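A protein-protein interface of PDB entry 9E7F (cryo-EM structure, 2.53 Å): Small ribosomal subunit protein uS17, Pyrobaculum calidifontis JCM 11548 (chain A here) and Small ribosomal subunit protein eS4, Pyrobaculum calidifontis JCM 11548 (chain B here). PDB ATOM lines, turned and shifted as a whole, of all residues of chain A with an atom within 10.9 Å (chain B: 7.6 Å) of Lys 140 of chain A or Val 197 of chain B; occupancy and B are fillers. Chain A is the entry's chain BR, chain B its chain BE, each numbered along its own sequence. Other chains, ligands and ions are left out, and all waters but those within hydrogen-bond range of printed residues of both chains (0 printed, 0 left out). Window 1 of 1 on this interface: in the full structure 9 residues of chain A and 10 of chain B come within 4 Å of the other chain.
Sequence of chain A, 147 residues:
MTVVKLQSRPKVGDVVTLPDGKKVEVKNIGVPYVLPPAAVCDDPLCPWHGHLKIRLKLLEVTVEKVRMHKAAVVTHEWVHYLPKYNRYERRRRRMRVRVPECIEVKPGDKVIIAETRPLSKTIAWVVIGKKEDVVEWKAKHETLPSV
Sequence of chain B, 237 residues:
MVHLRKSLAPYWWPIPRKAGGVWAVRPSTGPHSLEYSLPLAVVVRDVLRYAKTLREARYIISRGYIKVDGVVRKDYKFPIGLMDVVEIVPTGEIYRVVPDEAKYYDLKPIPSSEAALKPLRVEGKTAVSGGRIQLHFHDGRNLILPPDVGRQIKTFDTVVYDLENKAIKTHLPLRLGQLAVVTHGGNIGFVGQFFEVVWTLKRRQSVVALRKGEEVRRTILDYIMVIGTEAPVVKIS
O of Phe 195 of chain B sits at hydrogen-bond distance from N of Leu 144 of chain A, 2.7 Å away.
The side-chain carboxylate of Glu 196 of chain B sits at hydrogen-bond distance from a ring nitrogen (NE2) of His 141 of chain A (3.5 Å).
The side-chain carboxylate (OE2) of Glu 196 of chain B lies close to the side-chain hydroxyl (OG1) of Thr 143 of chain A (3.2 Å).
O of Glu 142 of chain A is in hydrogen-bond range of N of Val 197 of chain B, at 3.1 Å.
O of Lys 140 of chain A sits at hydrogen-bond distance from N of Trp 199 of chain B (2.8 Å).
The indole nitrogen (NE1) of Trp 199 of chain B sits close to the side-chain carboxylate (OE1) of Glu 142 of chain A.
O of Val 197 of chain B sits close to O of Lys 140 of chain A (3.2 Å).
The backbone NH (N) of Phe 195 of chain B lies within hydrogen-bond range of the backbone carbonyl oxygen (O) of Ala 209 of chain B, 3.4 Å away.
The backbone carbonyl oxygen (O) of Glu 196 of chain B is in hydrogen-bond range of the backbone NH (N) of Ala 209 of chain B (3.0 Å).
The backbone NH of Val 198 of chain B sits at hydrogen-bond distance from the backbone carbonyl oxygen of Val 207 of chain B (2.8 Å).
Of chain B, only Val 197, Val 198 and Trp 199 come within 4 Å of Lys 140 of chain A.
Of the printed residues of chain A, Leu 176 of chain B touches Glu 142 and Leu 144.
Printed residues of chain A within 4 Å of Phe 195 of chain B: Glu 142 (3.96 Å), Thr 143 (3.1 Å) and Leu 144 (2.7 Å).
Of chain A, only His 141, Glu 142 and Thr 143 come within 4 Å of Glu 196 of chain B.
Val 198 of chain B touches just these residues of chain A: Ala 139, Lys 140 and His 141.
Arg 203 of chain B touches none of the printed residues of chain A.
No residue of chain A comes within 4 Å of Val 207 of chain B.
No residue of chain A comes within 4 Å of Ala 209 of chain B.
The nearest residue of chain B that does not touch Lys 140 of chain A is Thr 200 of chain B (5.7 Å).
The nearest residue of chain A that does not touch Val 197 of chain B is Thr 143 of chain A (5.1 Å).
Among the printed residues, pairs that only touch across the chains: Lys 140 of chain A with Val 198 of chain B, Ala 139 of chain A with Trp 199 of chain B, Thr 143 of chain A with Phe 195 of chain B, Glu 142 of chain A with Glu 196 of chain B, His 141 of chain A with Val 197 of chain B, Leu 144 of chain A with Leu 176 of chain B, Glu 142 of chain A with Leu 176 of chain B, His 141 of chain A with Val 198 of chain B, Ala 139 of chain A with Val 198 of chain B and Glu 142 of chain A with Phe 195 of chain B.
Printed residues of chain A that touch a printed residue of chain B: Ala 139, Lys 140, His 141, Glu 142, Thr 143 and Leu 144.
Of the 16 printed residues of chain B, 6 touch a printed residue of chain A.
Printed residues of chain B that touch a printed residue of chain A: Leu 176, Phe 195, Glu 196, Val 197, Val 198 and Trp 199.
Among the printed residues, no Asp or Glu carboxylate lies within 4 Å of a Lys or Arg side-chain nitrogen of the other chain.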
ATOM      1  N   PRO A  32     -27.989   5.113  -7.697  1.00  0.00           N
ATOM      2  CA  PRO A  32     -27.021   4.747  -6.659  1.00  0.00           C
ATOM      3  C   PRO A  32     -26.659   5.855  -5.683  1.00  0.00           C
ATOM      4  O   PRO A  32     -25.837   5.613  -4.795  1.00  0.00           O
ATOM      5  CB  PRO A  32     -25.797   4.348  -7.488  1.00  0.00           C
ATOM      6  CG  PRO A  32     -25.890   5.194  -8.716  1.00  0.00           C
ATOM      7  CD  PRO A  32     -27.330   5.559  -8.935  1.00  0.00           C
ATOM      8  N   TRP A 137     -21.863  11.213  -5.477  1.00  0.00           N
ATOM      9  CA  TRP A 137     -21.588  10.174  -6.451  1.00  0.00           C
ATOM     10  C   TRP A 137     -20.753  10.745  -7.581  1.00  0.00           C
ATOM     11  O   TRP A 137     -20.961  11.882  -8.012  1.00  0.00           O
ATOM     12  CB  TRP A 137     -22.880   9.583  -7.004  1.00  0.00           C
ATOM     13  CG  TRP A 137     -22.679   8.298  -7.715  1.00  0.00           C
ATOM     14  CD1 TRP A 137     -22.469   7.079  -7.152  1.00  0.00           C
ATOM     15  CD2 TRP A 137     -22.669   8.096  -9.130  1.00  0.00           C
ATOM     16  NE1 TRP A 137     -22.328   6.125  -8.129  1.00  0.00           N
ATOM     17  CE2 TRP A 137     -22.446   6.726  -9.353  1.00  0.00           C
ATOM     18  CE3 TRP A 137     -22.823   8.944 -10.231  1.00  0.00           C
ATOM     19  CZ2 TRP A 137     -22.376   6.183 -10.628  1.00  0.00           C
ATOM     20  CZ3 TRP A 137     -22.755   8.404 -11.493  1.00  0.00           C
ATOM     21  CH2 TRP A 137     -22.534   7.036 -11.683  1.00  0.00           C
ATOM     22  N   LYS A 138     -19.808   9.949  -8.057  1.00  0.00           N
ATOM     23  CA  LYS A 138     -18.954  10.334  -9.165  1.00  0.00           C
ATOM     24  C   LYS A 138     -18.875   9.186 -10.155  1.00  0.00           C
ATOM     25  O   LYS A 138     -19.013   8.017  -9.789  1.00  0.00           O
ATOM     26  CB  LYS A 138     -17.554  10.711  -8.682  1.00  0.00           C
ATOM     27  CG  LYS A 138     -17.351  12.204  -8.497  1.00  0.00           C
ATOM     28  CD  LYS A 138     -16.764  12.843  -9.743  1.00  0.00           C
ATOM     29  CE  LYS A 138     -17.448  14.159 -10.057  1.00  0.00           C
ATOM     30  NZ  LYS A 138     -17.169  14.605 -11.445  1.00  0.00           N
ATOM     31  N   ALA A 139     -18.648   9.531 -11.416  1.00  0.00           N
ATOM     32  CA  ALA A 139     -18.475   8.530 -12.453  1.00  0.00           C
ATOM     33  C   ALA A 139     -17.085   7.907 -12.344  1.00  0.00           C
ATOM     34  O   ALA A 139     -16.352   8.108 -11.372  1.00  0.00           O
ATOM     35  CB  ALA A 139     -18.701   9.152 -13.828  1.00  0.00           C
ATOM     36  N   LYS A 140     -16.720   7.119 -13.347  1.00  0.00           N
ATOM     37  CA  LYS A 140     -15.402   6.513 -13.414  1.00  0.00           C
ATOM     38  C   LYS A 140     -14.648   7.071 -14.610  1.00  0.00           C
ATOM     39  O   LYS A 140     -15.220   7.237 -15.691  1.00  0.00           O
ATOM     40  CB  LYS A 140     -15.502   4.994 -13.507  1.00  0.00           C
ATOM     41  CG  LYS A 140     -16.429   4.390 -12.468  1.00  0.00           C
ATOM     42  CD  LYS A 140     -15.694   4.103 -11.171  1.00  0.00           C
ATOM     43  CE  LYS A 140     -16.342   2.962 -10.408  1.00  0.00           C
ATOM     44  NZ  LYS A 140     -16.936   1.946 -11.313  1.00  0.00           N
ATOM     45  N   HIS A 141     -13.367   7.368 -14.412  1.00  0.00           N
ATOM     46  CA  HIS A 141     -12.561   8.043 -15.427  1.00  0.00           C
ATOM     47  C   HIS A 141     -11.287   7.243 -15.666  1.00  0.00           C
ATOM     48  O   HIS A 141     -10.227   7.584 -15.137  1.00  0.00           O
ATOM     49  CB  HIS A 141     -12.257   9.466 -14.992  1.00  0.00           C
ATOM     50  CG  HIS A 141     -12.008  10.402 -16.128  1.00  0.00           C
ATOM     51  ND1 HIS A 141     -12.133  11.768 -16.006  1.00  0.00           N
ATOM     52  CD2 HIS A 141     -11.637  10.170 -17.408  1.00  0.00           C
ATOM     53  CE1 HIS A 141     -11.853  12.337 -17.165  1.00  0.00           C
ATOM     54  NE2 HIS A 141     -11.549  11.390 -18.032  1.00  0.00           N
ATOM     55  N   GLU A 142     -11.379   6.201 -16.484  1.00  0.00           N
ATOM     56  CA  GLU A 142     -10.232   5.364 -16.800  1.00  0.00           C
ATOM     57  C   GLU A 142      -9.540   5.907 -18.040  1.00  0.00           C
ATOM     58  O   GLU A 142     -10.194   6.193 -19.046  1.00  0.00           O
ATOM     59  CB  GLU A 142     -10.624   3.900 -17.018  1.00  0.00           C
ATOM     60  CG  GLU A 142     -11.118   3.121 -15.779  1.00  0.00           C
ATOM     61  CD  GLU A 142     -12.489   3.531 -15.271  1.00  0.00           C
ATOM     62  OE1 GLU A 142     -13.389   2.669 -15.269  1.00  0.00           O
ATOM     63  OE2 GLU A 142     -12.665   4.692 -14.852  1.00  0.00           O
ATOM     64  N   THR A 143      -8.221   6.052 -17.960  1.00  0.00           N
ATOM     65  CA  THR A 143      -7.437   6.632 -19.037  1.00  0.00           C
ATOM     66  C   THR A 143      -6.193   5.791 -19.270  1.00  0.00           C
ATOM     67  O   THR A 143      -5.513   5.395 -18.320  1.00  0.00           O
ATOM     68  CB  THR A 143      -7.042   8.075 -18.712  1.00  0.00           C
ATOM     69  OG1 THR A 143      -8.136   8.946 -19.012  1.00  0.00           O
ATOM     70  CG2 THR A 143      -5.842   8.507 -19.535  1.00  0.00           C
ATOM     71  N   LEU A 144      -5.906   5.511 -20.534  1.00  0.00           N
ATOM     72  CA  LEU A 144      -4.671   4.834 -20.895  1.00  0.00           C
ATOM     73  C   LEU A 144      -3.568   5.868 -21.071  1.00  0.00           C
ATOM     74  O   LEU A 144      -3.702   6.756 -21.923  1.00  0.00           O
ATOM     75  CB  LEU A 144      -4.852   4.039 -22.171  1.00  0.00           C
ATOM     76  CG  LEU A 144      -5.389   2.629 -21.955  1.00  0.00           C
ATOM     77  CD1 LEU A 144      -5.256   1.825 -23.225  1.00  0.00           C
ATOM     78  CD2 LEU A 144      -4.648   1.960 -20.822  1.00  0.00           C
ATOM     79  N   PRO A 145      -2.477   5.800 -20.296  1.00  0.00           N
ATOM     80  CA  PRO A 145      -1.374   6.770 -20.308  1.00  0.00           C
ATOM     81  C   PRO A 145      -0.706   6.934 -21.670  1.00  0.00           C
ATOM     82  O   PRO A 145      -0.756   6.019 -22.490  1.00  0.00           O
ATOM     83  CB  PRO A 145      -0.387   6.184 -19.292  1.00  0.00           C
ATOM     84  CG  PRO A 145      -0.773   4.750 -19.153  1.00  0.00           C
ATOM     85  CD  PRO A 145      -2.249   4.728 -19.316  1.00  0.00           C
ATOM     86  N   LEU B 174     -14.854  -4.681 -26.447  1.00  0.00           N
ATOM     87  CA  LEU B 174     -14.687  -3.248 -26.216  1.00  0.00           C
ATOM     88  C   LEU B 174     -13.897  -3.055 -24.930  1.00  0.00           C
ATOM     89  O   LEU B 174     -14.447  -3.054 -23.827  1.00  0.00           O
ATOM     90  CB  LEU B 174     -16.034  -2.546 -26.142  1.00  0.00           C
ATOM     91  CG  LEU B 174     -15.947  -1.053 -25.825  1.00  0.00           C
ATOM     92  CD1 LEU B 174     -15.820  -0.233 -27.098  1.00  0.00           C
ATOM     93  CD2 LEU B 174     -17.131  -0.596 -24.995  1.00  0.00           C
ATOM     94  N   LEU B 176     -10.388  -0.651 -23.309  1.00  0.00           N
ATOM     95  CA  LEU B 176      -9.567   0.530 -23.511  1.00  0.00           C
ATOM     96  C   LEU B 176      -8.276   0.152 -24.218  1.00  0.00           C
ATOM     97  O   LEU B 176      -7.594  -0.796 -23.822  1.00  0.00           O
ATOM     98  CB  LEU B 176      -9.263   1.173 -22.164  1.00  0.00           C
ATOM     99  CG  LEU B 176     -10.147   2.343 -21.753  1.00  0.00           C
ATOM    100  CD1 LEU B 176      -9.782   2.794 -20.354  1.00  0.00           C
ATOM    101  CD2 LEU B 176     -10.014   3.473 -22.737  1.00  0.00           C
ATOM    102  N   PHE B 194      -8.756   4.092 -28.533  1.00  0.00           N
ATOM    103  CA  PHE B 194      -9.633   4.251 -27.379  1.00  0.00           C
ATOM    104  C   PHE B 194      -8.761   4.319 -26.131  1.00  0.00           C
ATOM    105  O   PHE B 194      -8.107   3.339 -25.770  1.00  0.00           O
ATOM    106  CB  PHE B 194     -10.615   3.088 -27.305  1.00  0.00           C
ATOM    107  CG  PHE B 194     -11.763   3.313 -26.374  1.00  0.00           C
ATOM    108  CD1 PHE B 194     -12.098   4.582 -25.956  1.00  0.00           C
ATOM    109  CD2 PHE B 194     -12.509   2.249 -25.922  1.00  0.00           C
ATOM    110  CE1 PHE B 194     -13.149   4.785 -25.100  1.00  0.00           C
ATOM    111  CE2 PHE B 194     -13.564   2.444 -25.067  1.00  0.00           C
ATOM    112  CZ  PHE B 194     -13.885   3.714 -24.655  1.00  0.00           C
ATOM    113  N   PHE B 195      -8.755   5.473 -25.469  1.00  0.00           N
ATOM    114  CA  PHE B 195      -7.855   5.681 -24.346  1.00  0.00           C
ATOM    115  C   PHE B 195      -8.490   6.365 -23.147  1.00  0.00           C
ATOM    116  O   PHE B 195      -7.787   6.608 -22.163  1.00  0.00           O
ATOM    117  CB  PHE B 195      -6.631   6.492 -24.796  1.00  0.00           C
ATOM    118  CG  PHE B 195      -6.910   7.951 -25.020  1.00  0.00           C
ATOM    119  CD1 PHE B 195      -7.576   8.377 -26.151  1.00  0.00           C
ATOM    120  CD2 PHE B 195      -6.493   8.897 -24.106  1.00  0.00           C
ATOM    121  CE1 PHE B 195      -7.829   9.711 -26.362  1.00  0.00           C
ATOM    122  CE2 PHE B 195      -6.746  10.233 -24.315  1.00  0.00           C
ATOM    123  CZ  PHE B 195      -7.413  10.638 -25.444  1.00  0.00           C
ATOM    124  N   GLU B 196      -9.780   6.677 -23.183  1.00  0.00           N
ATOM    125  CA  GLU B 196     -10.397   7.431 -22.104  1.00  0.00           C
ATOM    126  C   GLU B 196     -11.896   7.192 -22.123  1.00  0.00           C
ATOM    127  O   GLU B 196     -12.513   7.186 -23.188  1.00  0.00           O
ATOM    128  CB  GLU B 196     -10.098   8.924 -22.246  1.00  0.00           C
ATOM    129  CG  GLU B 196     -10.265   9.721 -20.980  1.00  0.00           C
ATOM    130  CD  GLU B 196      -9.860  11.168 -21.161  1.00  0.00           C
ATOM    131  OE1 GLU B 196     -10.373  11.819 -22.095  1.00  0.00           O
ATOM    132  OE2 GLU B 196      -9.023  11.657 -20.373  1.00  0.00           O
ATOM    133  N   VAL B 197     -12.471   7.000 -20.942  1.00  0.00           N
ATOM    134  CA  VAL B 197     -13.912   6.823 -20.815  1.00  0.00           C
ATOM    135  C   VAL B 197     -14.356   7.382 -19.475  1.00  0.00           C
ATOM    136  O   VAL B 197     -13.694   7.180 -18.453  1.00  0.00           O
ATOM    137  CB  VAL B 197     -14.331   5.347 -20.959  1.00  0.00           C
ATOM    138  CG1 VAL B 197     -13.775   4.521 -19.823  1.00  0.00           C
ATOM    139  CG2 VAL B 197     -15.838   5.237 -21.010  1.00  0.00           C
ATOM    140  N   VAL B 198     -15.469   8.102 -19.488  1.00  0.00           N
ATOM    141  CA  VAL B 198     -16.145   8.542 -18.279  1.00  0.00           C
ATOM    142  C   VAL B 198     -17.428   7.728 -18.206  1.00  0.00           C
ATOM    143  O   VAL B 198     -18.415   8.044 -18.869  1.00  0.00           O
ATOM    144  CB  VAL B 198     -16.424  10.045 -18.289  1.00  0.00           C
ATOM    145  CG1 VAL B 198     -17.400  10.399 -17.192  1.00  0.00           C
ATOM    146  CG2 VAL B 198     -15.138  10.815 -18.111  1.00  0.00           C
ATOM    147  N   TRP B 199     -17.411   6.665 -17.411  1.00  0.00           N
ATOM    148  CA  TRP B 199     -18.549   5.758 -17.347  1.00  0.00           C
ATOM    149  C   TRP B 199     -19.709   6.453 -16.655  1.00  0.00           C
ATOM    150  O   TRP B 199     -19.639   6.757 -15.462  1.00  0.00           O
ATOM    151  CB  TRP B 199     -18.165   4.482 -16.610  1.00  0.00           C
ATOM    152  CG  TRP B 199     -17.227   3.620 -17.372  1.00  0.00           C
ATOM    153  CD1 TRP B 199     -15.935   3.339 -17.052  1.00  0.00           C
ATOM    154  CD2 TRP B 199     -17.503   2.914 -18.584  1.00  0.00           C
ATOM    155  NE1 TRP B 199     -15.388   2.500 -17.987  1.00  0.00           N
ATOM    156  CE2 TRP B 199     -16.331   2.225 -18.940  1.00  0.00           C
ATOM    157  CE3 TRP B 199     -18.629   2.796 -19.402  1.00  0.00           C
ATOM    158  CZ2 TRP B 199     -16.250   1.435 -20.076  1.00  0.00           C
ATOM    159  CZ3 TRP B 199     -18.547   2.009 -20.530  1.00  0.00           C
ATOM    160  CH2 TRP B 199     -17.368   1.339 -20.855  1.00  0.00           C
ATOM    161  N   THR B 200     -20.772   6.706 -17.399  1.00  0.00           N
ATOM    162  CA  THR B 200     -21.973   7.302 -16.847  1.00  0.00           C
ATOM    163  C   THR B 200     -22.891   6.223 -16.285  1.00  0.00           C
ATOM    164  O   THR B 200     -22.594   5.028 -16.331  1.00  0.00           O
ATOM    165  CB  THR B 200     -22.694   8.121 -17.913  1.00  0.00           C
ATOM    166  OG1 THR B 200     -22.677   7.405 -19.152  1.00  0.00           O
ATOM    167  CG2 THR B 200     -22.011   9.455 -18.099  1.00  0.00           C
ATOM    168  N   ARG B 203     -24.739   3.247 -19.736  1.00  0.00           N
ATOM    169  CA  ARG B 203     -23.492   2.887 -20.402  1.00  0.00           C
ATOM    170  C   ARG B 203     -23.470   3.378 -21.840  1.00  0.00           C
ATOM    171  O   ARG B 203     -22.414   3.748 -22.363  1.00  0.00           O
ATOM    172  CB  ARG B 203     -23.292   1.376 -20.359  1.00  0.00           C
ATOM    173  CG  ARG B 203     -22.827   0.844 -19.018  1.00  0.00           C
ATOM    174  CD  ARG B 203     -22.633  -0.661 -19.072  1.00  0.00           C
ATOM    175  NE  ARG B 203     -21.719  -1.051 -20.137  1.00  0.00           N
ATOM    176  CZ  ARG B 203     -20.414  -1.215 -19.983  1.00  0.00           C
ATOM    177  NH1 ARG B 203     -19.829  -1.035 -18.811  1.00  0.00           N
ATOM    178  NH2 ARG B 203     -19.674  -1.563 -21.032  1.00  0.00           N
ATOM    179  N   GLN B 205     -24.471   6.119 -22.911  1.00  0.00           N
ATOM    180  CA  GLN B 205     -24.189   7.542 -22.909  1.00  0.00           C
ATOM    181  C   GLN B 205     -22.817   7.867 -22.339  1.00  0.00           C
ATOM    182  O   GLN B 205     -22.549   9.030 -22.030  1.00  0.00           O
ATOM    183  CB  GLN B 205     -25.268   8.280 -22.119  1.00  0.00           C
ATOM    184  CG  GLN B 205     -26.631   8.215 -22.760  1.00  0.00           C
ATOM    185  CD  GLN B 205     -26.676   8.954 -24.077  1.00  0.00           C
ATOM    186  OE1 GLN B 205     -25.998   9.962 -24.259  1.00  0.00           O
ATOM    187  NE2 GLN B 205     -27.478   8.454 -25.005  1.00  0.00           N
ATOM    188  N   SER B 206     -21.954   6.872 -22.173  1.00  0.00           N
ATOM    189  CA  SER B 206     -20.634   7.116 -21.615  1.00  0.00           C
ATOM    190  C   SER B 206     -19.791   7.948 -22.570  1.00  0.00           C
ATOM    191  O   SER B 206     -19.859   7.796 -23.790  1.00  0.00           O
ATOM    192  CB  SER B 206     -19.930   5.798 -21.317  1.00  0.00           C
ATOM    193  OG  SER B 206     -20.839   4.852 -20.792  1.00  0.00           O
ATOM    194  N   VAL B 207     -18.991   8.840 -22.001  1.00  0.00           N
ATOM    195  CA  VAL B 207     -18.129   9.716 -22.782  1.00  0.00           C
ATOM    196  C   VAL B 207     -16.837   8.975 -23.082  1.00  0.00           C
ATOM    197  O   VAL B 207     -16.160   8.495 -22.169  1.00  0.00           O
ATOM    198  CB  VAL B 207     -17.850  11.029 -22.040  1.00  0.00           C
ATOM    199  CG1 VAL B 207     -17.222  12.032 -22.982  1.00  0.00           C
ATOM    200  CG2 VAL B 207     -19.129  11.577 -21.455  1.00  0.00           C
ATOM    201  N   VAL B 208     -16.491   8.890 -24.361  1.00  0.00           N
ATOM    202  CA  VAL B 208     -15.330   8.145 -24.822  1.00  0.00           C
ATOM    203  C   VAL B 208     -14.461   9.070 -25.657  1.00  0.00           C
ATOM    204  O   VAL B 208     -14.970   9.951 -26.356  1.00  0.00           O
ATOM    205  CB  VAL B 208     -15.749   6.903 -25.631  1.00  0.00           C
ATOM    206  CG1 VAL B 208     -16.678   6.042 -24.812  1.00  0.00           C
ATOM    207  CG2 VAL B 208     -16.418   7.322 -26.917  1.00  0.00           C
ATOM    208  N   ALA B 209     -13.149   8.869 -25.581  1.00  0.00           N
ATOM    209  CA  ALA B 209     -12.180   9.702 -26.278  1.00  0.00           C
ATOM    210  C   ALA B 209     -11.331   8.847 -27.205  1.00  0.00           C
ATOM    211  O   ALA B 209     -10.915   7.748 -26.832  1.00  0.00           O
ATOM    212  CB  ALA B 209     -11.287  10.444 -25.284  1.00  0.00           C
ATOM    213  N   LEU B 221     -20.328   6.546 -25.973  1.00  0.00           N
ATOM    214  CA  LEU B 221     -19.953   5.159 -26.222  1.00  0.00           C
ATOM    215  C   LEU B 221     -20.830   4.516 -27.285  1.00  0.00           C
ATOM    216  O   LEU B 221     -20.405   3.568 -27.951  1.00  0.00           O
ATOM    217  CB  LEU B 221     -20.025   4.359 -24.927  1.00  0.00           C
ATOM    218  CG  LEU B 221     -20.025   2.840 -25.057  1.00  0.00           C
ATOM    219  CD1 LEU B 221     -18.749   2.376 -25.712  1.00  0.00           C
ATOM    220  CD2 LEU B 221     -20.187   2.192 -23.700  1.00  0.00           C
